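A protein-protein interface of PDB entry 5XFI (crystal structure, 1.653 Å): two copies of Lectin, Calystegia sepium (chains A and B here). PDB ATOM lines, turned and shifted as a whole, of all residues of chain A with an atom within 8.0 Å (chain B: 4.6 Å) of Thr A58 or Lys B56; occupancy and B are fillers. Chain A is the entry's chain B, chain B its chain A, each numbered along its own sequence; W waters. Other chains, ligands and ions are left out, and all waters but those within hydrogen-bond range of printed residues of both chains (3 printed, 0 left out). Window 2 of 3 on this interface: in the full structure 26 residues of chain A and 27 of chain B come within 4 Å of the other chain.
N of Thr A60 is in hydrogen-bond range of OD1 of Asp B57 (2.9 Å).
O of Thr B58 sits at hydrogen-bond distance from N of Thr A58, 2.9 Å away.
Of the 10 printed residues of chain B, 4 touch a printed residue of chain A.
Of the 18 printed residues of chain A, 6 touch a printed residue of chain B.
Lys A56 touches Thr B58, and with the chains exchanged Thr A58 touches Lys B56.
Asp A57 touches Thr B58, and with the chains exchanged Thr A58 touches Asp B57.
Thr A58 touches its own counterpart, Thr B58.
NZ of Lys B56 is in hydrogen-bond range of OE1 of Gln B30 (2.9 Å).
The side-chain hydroxyl (OG) of Ser B48 is in hydrogen-bond range of the side-chain hydroxyl (OG1) of Thr B58.
O of Ser B49 sits at hydrogen-bond distance from N of Asp B57 (2.8 Å).
NZ of Lys A56 lies within hydrogen-bond range of OE1 of Gln A30.
O of Phe A47 sits close to OG1 of Thr A58.
The backbone carbonyl oxygen (O) of Ile A59 is in hydrogen-bond range of the backbone NH (N) of Phe A47, 3.0 Å away.
Thr A58 touches just these residues of chain B: Lys B56, Asp B57 and Thr B58.
Ser B55 touches none of the printed residues of chain A.
Of chain A, only Thr A58 comes within 4 Å of Lys B56.
Of the printed residues of chain A, Asp B57 touches Thr A58, Ile A59 and Thr A60.
Of the printed residues of chain A, Thr B58 touches Lys A56, Asp A57 and Thr A58.
The nearest residue of chain A that does not touch Lys B56 is Ile A59 (5.9 Å).
The nearest printed residue of chain B that does not touch Thr A60 is Ser B55 (5.0 Å).
Phe B22 touches Ser A21.
CG2 of Thr B58 touches O of Lys A56, 3.3 Å away.
O of Thr B58 touches CA of Asp A57, 3.3 Å away.
CG2 of Thr A58 touches O of Lys B56 (3.2 Å).
Thr A58 touches Asp B57.
Asp B57 touches Ile A59.
Water W2 lies within hydrogen-bond range of the side-chain carboxylate of Asp B57 and the backbone carbonyl oxygen of Thr A60.
Water W3 lies within hydrogen-bond range of OG1 of Thr A60, OG1 of Thr A58 and OD1 of Asp B57.
Water W1 bridges OG1 of Thr B58 (2.9 Å) and OD1 of Asp A57 (3.4 Å).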
ATOM      1  N   SER A  21       6.204  27.049 -11.512  1.00  0.00           N
ATOM      2  CA  SER A  21       5.190  26.040 -11.811  1.00  0.00           C
ATOM      3  C   SER A  21       5.852  24.784 -12.367  1.00  0.00           C
ATOM      4  O   SER A  21       6.775  24.863 -13.189  1.00  0.00           O
ATOM      5  CB  SER A  21       4.165  26.593 -12.813  1.00  0.00           C
ATOM      6  OG  SER A  21       3.155  25.615 -13.123  1.00  0.00           O
ATOM      7  N   PHE A  22       5.362  23.621 -11.926  1.00  0.00           N
ATOM      8  CA  PHE A  22       5.921  22.353 -12.395  1.00  0.00           C
ATOM      9  C   PHE A  22       4.838  21.286 -12.388  1.00  0.00           C
ATOM     10  O   PHE A  22       4.484  20.772 -11.322  1.00  0.00           O
ATOM     11  CB  PHE A  22       7.076  21.946 -11.497  1.00  0.00           C
ATOM     12  CG  PHE A  22       7.763  20.668 -11.908  1.00  0.00           C
ATOM     13  CD1 PHE A  22       8.565  20.620 -13.054  1.00  0.00           C
ATOM     14  CD2 PHE A  22       7.668  19.528 -11.102  1.00  0.00           C
ATOM     15  CE1 PHE A  22       9.260  19.428 -13.409  1.00  0.00           C
ATOM     16  CE2 PHE A  22       8.332  18.339 -11.448  1.00  0.00           C
ATOM     17  CZ  PHE A  22       9.126  18.285 -12.618  1.00  0.00           C
ATOM     18  N   PRO A  24       4.733  17.911 -14.485  1.00  0.00           N
ATOM     19  CA  PRO A  24       5.312  17.012 -15.488  1.00  0.00           C
ATOM     20  C   PRO A  24       4.271  15.993 -15.944  1.00  0.00           C
ATOM     21  O   PRO A  24       3.257  15.773 -15.283  1.00  0.00           O
ATOM     22  CB  PRO A  24       6.454  16.334 -14.702  1.00  0.00           C
ATOM     23  CG  PRO A  24       5.891  16.235 -13.264  1.00  0.00           C
ATOM     24  CD  PRO A  24       5.112  17.558 -13.102  1.00  0.00           C
ATOM     25  N   GLN A  30       9.989  11.844  -6.642  1.00  0.00           N
ATOM     26  CA  GLN A  30      10.976  12.149  -5.618  1.00  0.00           C
ATOM     27  C   GLN A  30      10.943  13.640  -5.349  1.00  0.00           C
ATOM     28  O   GLN A  30      10.766  14.446  -6.272  1.00  0.00           O
ATOM     29  CB  GLN A  30      12.385  11.628  -5.986  1.00  0.00           C
ATOM     30  CG  GLN A  30      13.249  12.407  -6.908  1.00  0.00           C
ATOM     31  CD  GLN A  30      14.676  11.807  -7.089  1.00  0.00           C
ATOM     32  OE1 GLN A  30      15.579  12.517  -7.522  1.00  0.00           O
ATOM     33  NE2 GLN A  30      14.862  10.504  -6.797  1.00  0.00           N
ATOM     34  N   VAL A  32      12.829  16.679  -2.699  1.00  0.00           N
ATOM     35  CA  VAL A  32      13.889  17.046  -1.764  1.00  0.00           C
ATOM     36  C   VAL A  32      13.463  18.312  -1.055  1.00  0.00           C
ATOM     37  O   VAL A  32      13.153  19.308  -1.718  1.00  0.00           O
ATOM     38  CB  VAL A  32      15.239  17.302  -2.454  1.00  0.00           C
ATOM     39  CG1 VAL A  32      16.329  17.566  -1.394  1.00  0.00           C
ATOM     40  CG2 VAL A  32      15.600  16.170  -3.366  1.00  0.00           C
ATOM     41  N   LEU A  45      12.735  23.611  -2.393  1.00  0.00           N
ATOM     42  CA  LEU A  45      12.019  22.373  -2.697  1.00  0.00           C
ATOM     43  C   LEU A  45      12.421  21.916  -4.081  1.00  0.00           C
ATOM     44  O   LEU A  45      12.556  22.722  -5.008  1.00  0.00           O
ATOM     45  CB  LEU A  45      10.481  22.537  -2.653  1.00  0.00           C
ATOM     46  CG  LEU A  45       9.842  22.886  -1.302  1.00  0.00           C
ATOM     47  CD1 LEU A  45       8.393  23.310  -1.510  1.00  0.00           C
ATOM     48  CD2 LEU A  45       9.978  21.721  -0.271  1.00  0.00           C
ATOM     49  N   THR A  46      12.635  20.615  -4.219  1.00  0.00           N
ATOM     50  CA  THR A  46      12.925  20.008  -5.506  1.00  0.00           C
ATOM     51  C   THR A  46      11.844  18.971  -5.769  1.00  0.00           C
ATOM     52  O   THR A  46      11.546  18.159  -4.897  1.00  0.00           O
ATOM     53  CB  THR A  46      14.317  19.331  -5.511  1.00  0.00           C
ATOM     54  OG1 THR A  46      15.362  20.282  -5.249  1.00  0.00           O
ATOM     55  CG2 THR A  46      14.591  18.640  -6.856  1.00  0.00           C
ATOM     56  N   PHE A  47      11.268  18.985  -6.962  1.00  0.00           N
ATOM     57  CA  PHE A  47      10.305  17.968  -7.377  1.00  0.00           C
ATOM     58  C   PHE A  47      10.835  17.312  -8.639  1.00  0.00           C
ATOM     59  O   PHE A  47      11.274  18.015  -9.554  1.00  0.00           O
ATOM     60  CB  PHE A  47       8.921  18.571  -7.670  1.00  0.00           C
ATOM     61  CG  PHE A  47       8.355  19.382  -6.553  1.00  0.00           C
ATOM     62  CD1 PHE A  47       7.763  18.765  -5.452  1.00  0.00           C
ATOM     63  CD2 PHE A  47       8.388  20.764  -6.621  1.00  0.00           C
ATOM     64  CE1 PHE A  47       7.235  19.506  -4.424  1.00  0.00           C
ATOM     65  CE2 PHE A  47       7.849  21.535  -5.613  1.00  0.00           C
ATOM     66  CZ  PHE A  47       7.291  20.918  -4.500  1.00  0.00           C
ATOM     67  N   SER A  48      10.802  15.974  -8.702  1.00  0.00           N
ATOM     68  CA  SER A  48      11.347  15.292  -9.868  1.00  0.00           C
ATOM     69  C   SER A  48      10.458  14.132 -10.279  1.00  0.00           C
ATOM     70  O   SER A  48       9.793  13.509  -9.452  1.00  0.00           O
ATOM     71  CB  SER A  48      12.773  14.760  -9.610  1.00  0.00           C
ATOM     72  OG  SER A  48      13.652  15.817  -9.275  1.00  0.00           O
ATOM     73  N   SER A  49      10.455  13.863 -11.581  1.00  0.00           N
ATOM     74  CA  SER A  49       9.669  12.809 -12.207  1.00  0.00           C
ATOM     75  C   SER A  49      10.583  12.056 -13.162  1.00  0.00           C
ATOM     76  O   SER A  49      11.120  12.642 -14.107  1.00  0.00           O
ATOM     77  CB  SER A  49       8.479  13.401 -12.966  1.00  0.00           C
ATOM     78  OG  SER A  49       7.797  12.388 -13.682  1.00  0.00           O
ATOM     79  N   THR A  50      10.757  10.763 -12.934  1.00  0.00           N
ATOM     80  CA  THR A  50      11.600   9.974 -13.818  1.00  0.00           C
ATOM     81  C   THR A  50      10.769   9.436 -14.974  1.00  0.00           C
ATOM     82  O   THR A  50       9.671   8.911 -14.764  1.00  0.00           O
ATOM     83  CB  THR A  50      12.279   8.846 -13.044  1.00  0.00           C
ATOM     84  OG1 THR A  50      13.235   9.421 -12.146  1.00  0.00           O
ATOM     85  CG2 THR A  50      13.015   7.922 -14.009  1.00  0.00           C
ATOM     86  N   SER A  55      15.232   9.862 -18.773  1.00  0.00           N
ATOM     87  CA  SER A  55      15.294  11.282 -18.494  1.00  0.00           C
ATOM     88  C   SER A  55      14.467  11.590 -17.251  1.00  0.00           C
ATOM     89  O   SER A  55      13.531  10.866 -16.893  1.00  0.00           O
ATOM     90  CB  SER A  55      14.796  12.098 -19.689  1.00  0.00           C
ATOM     91  OG  SER A  55      13.417  11.870 -19.915  1.00  0.00           O
ATOM     92  N   LYS A  56      14.812  12.696 -16.610  1.00  0.00           N
ATOM     93  CA  LYS A  56      14.231  13.065 -15.332  1.00  0.00           C
ATOM     94  C   LYS A  56      13.801  14.518 -15.403  1.00  0.00           C
ATOM     95  O   LYS A  56      14.648  15.420 -15.488  1.00  0.00           O
ATOM     96  CB  LYS A  56      15.248  12.835 -14.226  1.00  0.00           C
ATOM     97  CG  LYS A  56      14.800  13.096 -12.837  1.00  0.00           C
ATOM     98  CD  LYS A  56      16.009  12.775 -11.949  1.00  0.00           C
ATOM     99  CE  LYS A  56      15.637  12.486 -10.541  1.00  0.00           C
ATOM    100  NZ  LYS A  56      16.848  12.054  -9.766  1.00  0.00           N
ATOM    101  N   ASP A  57      12.490  14.742 -15.386  1.00  0.00           N
ATOM    102  CA  ASP A  57      11.974  16.100 -15.281  1.00  0.00           C
ATOM    103  C   ASP A  57      12.212  16.586 -13.859  1.00  0.00           C
ATOM    104  O   ASP A  57      12.039  15.828 -12.905  1.00  0.00           O
ATOM    105  CB  ASP A  57      10.475  16.125 -15.604  1.00  0.00           C
ATOM    106  CG  ASP A  57      10.150  15.734 -17.051  1.00  0.00           C
ATOM    107  OD1 ASP A  57      10.978  15.919 -17.962  1.00  0.00           O
ATOM    108  OD2 ASP A  57       9.015  15.245 -17.249  1.00  0.00           O
ATOM    109  N   THR A  58      12.635  17.839 -13.700  1.00  0.00           N
ATOM    110  CA  THR A  58      12.962  18.288 -12.349  1.00  0.00           C
ATOM    111  C   THR A  58      12.846  19.802 -12.263  1.00  0.00           C
ATOM    112  O   THR A  58      13.005  20.514 -13.258  1.00  0.00           O
ATOM    113  CB  THR A  58      14.365  17.817 -11.925  1.00  0.00           C
ATOM    114  OG1 THR A  58      14.561  18.092 -10.526  1.00  0.00           O
ATOM    115  CG2 THR A  58      15.437  18.527 -12.742  1.00  0.00           C
ATOM    116  N   ILE A  59      12.516  20.279 -11.069  1.00  0.00           N
ATOM    117  CA  ILE A  59      12.565  21.705 -10.784  1.00  0.00           C
ATOM    118  C   ILE A  59      13.064  21.856  -9.364  1.00  0.00           C
ATOM    119  O   ILE A  59      12.742  21.035  -8.501  1.00  0.00           O
ATOM    120  CB  ILE A  59      11.185  22.380 -10.976  1.00  0.00           C
ATOM    121  CG1 ILE A  59      11.355  23.896 -11.041  1.00  0.00           C
ATOM    122  CG2 ILE A  59      10.216  22.001  -9.834  1.00  0.00           C
ATOM    123  CD1 ILE A  59      10.087  24.642 -11.367  1.00  0.00           C
ATOM    124  N   THR A  60      13.865  22.895  -9.122  1.00  0.00           N
ATOM    125  CA  THR A  60      14.177  23.324  -7.763  1.00  0.00           C
ATOM    126  C   THR A  60      13.726  24.770  -7.593  1.00  0.00           C
ATOM    127  O   THR A  60      14.055  25.632  -8.424  1.00  0.00           O
ATOM    128  CB  THR A  60      15.666  23.177  -7.460  1.00  0.00           C
ATOM    129  OG1 THR A  60      15.993  21.784  -7.479  1.00  0.00           O
ATOM    130  CG2 THR A  60      15.987  23.743  -6.123  1.00  0.00           C
ATOM    131  N   VAL A  61      12.990  25.034  -6.517  1.00  0.00           N
ATOM    132  CA  VAL A  61      12.466  26.369  -6.256  1.00  0.00           C
ATOM    133  C   VAL A  61      12.883  26.777  -4.852  1.00  0.00           C
ATOM    134  O   VAL A  61      12.971  25.947  -3.946  1.00  0.00           O
ATOM    135  CB  VAL A  61      10.931  26.426  -6.445  1.00  0.00           C
ATOM    136  CG1 VAL A  61      10.582  26.028  -7.874  1.00  0.00           C
ATOM    137  CG2 VAL A  61      10.216  25.489  -5.473  1.00  0.00           C
ATOM    138  N   PHE B  22       5.561  24.304 -17.006  1.00  0.00           N
ATOM    139  CA  PHE B  22       6.966  24.477 -16.630  1.00  0.00           C
ATOM    140  C   PHE B  22       7.311  25.956 -16.605  1.00  0.00           C
ATOM    141  O   PHE B  22       7.533  26.557 -17.656  1.00  0.00           O
ATOM    142  CB  PHE B  22       7.860  23.747 -17.613  1.00  0.00           C
ATOM    143  CG  PHE B  22       9.322  23.788 -17.258  1.00  0.00           C
ATOM    144  CD1 PHE B  22       9.810  23.088 -16.153  1.00  0.00           C
ATOM    145  CD2 PHE B  22      10.226  24.481 -18.065  1.00  0.00           C
ATOM    146  CE1 PHE B  22      11.207  23.076 -15.862  1.00  0.00           C
ATOM    147  CE2 PHE B  22      11.596  24.504 -17.765  1.00  0.00           C
ATOM    148  CZ  PHE B  22      12.090  23.800 -16.658  1.00  0.00           C
ATOM    149  N   GLN B  30      17.683  26.655 -22.930  1.00  0.00           N
ATOM    150  CA  GLN B  30      17.937  25.505 -23.794  1.00  0.00           C
ATOM    151  C   GLN B  30      16.602  24.878 -24.152  1.00  0.00           C
ATOM    152  O   GLN B  30      15.809  24.594 -23.249  1.00  0.00           O
ATOM    153  CB  GLN B  30      18.825  24.497 -23.068  1.00  0.00           C
ATOM    154  CG  GLN B  30      19.306  23.285 -23.828  1.00  0.00           C
ATOM    155  CD  GLN B  30      20.377  22.527 -23.005  1.00  0.00           C
ATOM    156  OE1 GLN B  30      20.082  21.532 -22.341  1.00  0.00           O
ATOM    157  NE2 GLN B  30      21.610  23.034 -23.018  1.00  0.00           N
ATOM    158  N   SER B  48      14.740  23.697 -20.742  1.00  0.00           N
ATOM    159  CA  SER B  48      15.676  23.555 -19.638  1.00  0.00           C
ATOM    160  C   SER B  48      16.213  24.910 -19.214  1.00  0.00           C
ATOM    161  O   SER B  48      16.346  25.829 -20.027  1.00  0.00           O
ATOM    162  CB  SER B  48      16.864  22.623 -20.015  1.00  0.00           C
ATOM    163  OG  SER B  48      16.392  21.319 -20.358  1.00  0.00           O
ATOM    164  N   SER B  49      16.539  25.010 -17.928  1.00  0.00           N
ATOM    165  CA  SER B  49      17.054  26.225 -17.305  1.00  0.00           C
ATOM    166  C   SER B  49      18.217  25.834 -16.409  1.00  0.00           C
ATOM    167  O   SER B  49      18.041  25.065 -15.458  1.00  0.00           O
ATOM    168  CB  SER B  49      15.965  26.909 -16.482  1.00  0.00           C
ATOM    169  OG  SER B  49      16.498  28.022 -15.777  1.00  0.00           O
ATOM    170  N   THR B  50      19.405  26.353 -16.696  1.00  0.00           N
ATOM    171  CA  THR B  50      20.558  26.022 -15.876  1.00  0.00           C
ATOM    172  C   THR B  50      20.632  26.980 -14.696  1.00  0.00           C
ATOM    173  O   THR B  50      20.468  28.191 -14.863  1.00  0.00           O
ATOM    174  CB  THR B  50      21.843  26.049 -16.700  1.00  0.00           C
ATOM    175  OG1 THR B  50      21.803  24.973 -17.650  1.00  0.00           O
ATOM    176  CG2 THR B  50      23.040  25.840 -15.795  1.00  0.00           C
ATOM    177  N   GLY B  54      24.787  24.677 -10.819  1.00  0.00           N
ATOM    178  CA  GLY B  54      25.048  23.570 -11.718  1.00  0.00           C
ATOM    179  C   GLY B  54      23.895  22.616 -11.902  1.00  0.00           C
ATOM    180  O   GLY B  54      23.984  21.715 -12.746  1.00  0.00           O
ATOM    181  N   SER B  55      22.823  22.766 -11.134  1.00  0.00           N
ATOM    182  CA  SER B  55      21.632  21.982 -11.386  1.00  0.00           C
ATOM    183  C   SER B  55      20.874  22.577 -12.564  1.00  0.00           C
ATOM    184  O   SER B  55      21.023  23.754 -12.912  1.00  0.00           O
ATOM    185  CB  SER B  55      20.737  21.925 -10.146  1.00  0.00           C
ATOM    186  OG  SER B  55      20.177  23.199  -9.868  1.00  0.00           O
ATOM    187  N   LYS B  56      20.045  21.746 -13.174  1.00  0.00           N
ATOM    188  CA  LYS B  56      19.357  22.107 -14.401  1.00  0.00           C
ATOM    189  C   LYS B  56      17.891  21.729 -14.254  1.00  0.00           C
ATOM    190  O   LYS B  56      17.552  20.542 -14.161  1.00  0.00           O
ATOM    191  CB  LYS B  56      20.009  21.403 -15.590  1.00  0.00           C
ATOM    192  CG  LYS B  56      19.388  21.693 -16.929  1.00  0.00           C
ATOM    193  CD  LYS B  56      19.966  20.713 -17.931  1.00  0.00           C
ATOM    194  CE  LYS B  56      20.707  21.400 -19.019  1.00  0.00           C
ATOM    195  NZ  LYS B  56      21.314  20.396 -19.953  1.00  0.00           N
ATOM    196  N   ASP B  57      17.025  22.736 -14.206  1.00  0.00           N
ATOM    197  CA  ASP B  57      15.594  22.476 -14.255  1.00  0.00           C
ATOM    198  C   ASP B  57      15.233  22.057 -15.670  1.00  0.00           C
ATOM    199  O   ASP B  57      15.765  22.608 -16.636  1.00  0.00           O
ATOM    200  CB  ASP B  57      14.825  23.732 -13.850  1.00  0.00           C
ATOM    201  CG  ASP B  57      15.071  24.154 -12.400  1.00  0.00           C
ATOM    202  OD1 ASP B  57      15.386  23.307 -11.538  1.00  0.00           O
ATOM    203  OD2 ASP B  57      14.917  25.371 -12.151  1.00  0.00           O
ATOM    204  N   THR B  58      14.346  21.071 -15.807  1.00  0.00           N
ATOM    205  CA  THR B  58      14.059  20.565 -17.143  1.00  0.00           C
ATOM    206  C   THR B  58      12.707  19.859 -17.167  1.00  0.00           C
ATOM    207  O   THR B  58      12.241  19.320 -16.153  1.00  0.00           O
ATOM    208  CB  THR B  58      15.177  19.632 -17.640  1.00  0.00           C
ATOM    209  OG1 THR B  58      15.000  19.391 -19.048  1.00  0.00           O
ATOM    210  CG2 THR B  58      15.146  18.306 -16.898  1.00  0.00           C
HETATM  211  O   HOH W   1      13.606  16.985 -19.778  1.00  0.00           O
HETATM  212  O   HOH W   2      13.222  26.733 -10.843  1.00  0.00           O
HETATM  213  O   HOH W   3      15.983  20.432  -9.858  1.00  0.00           O
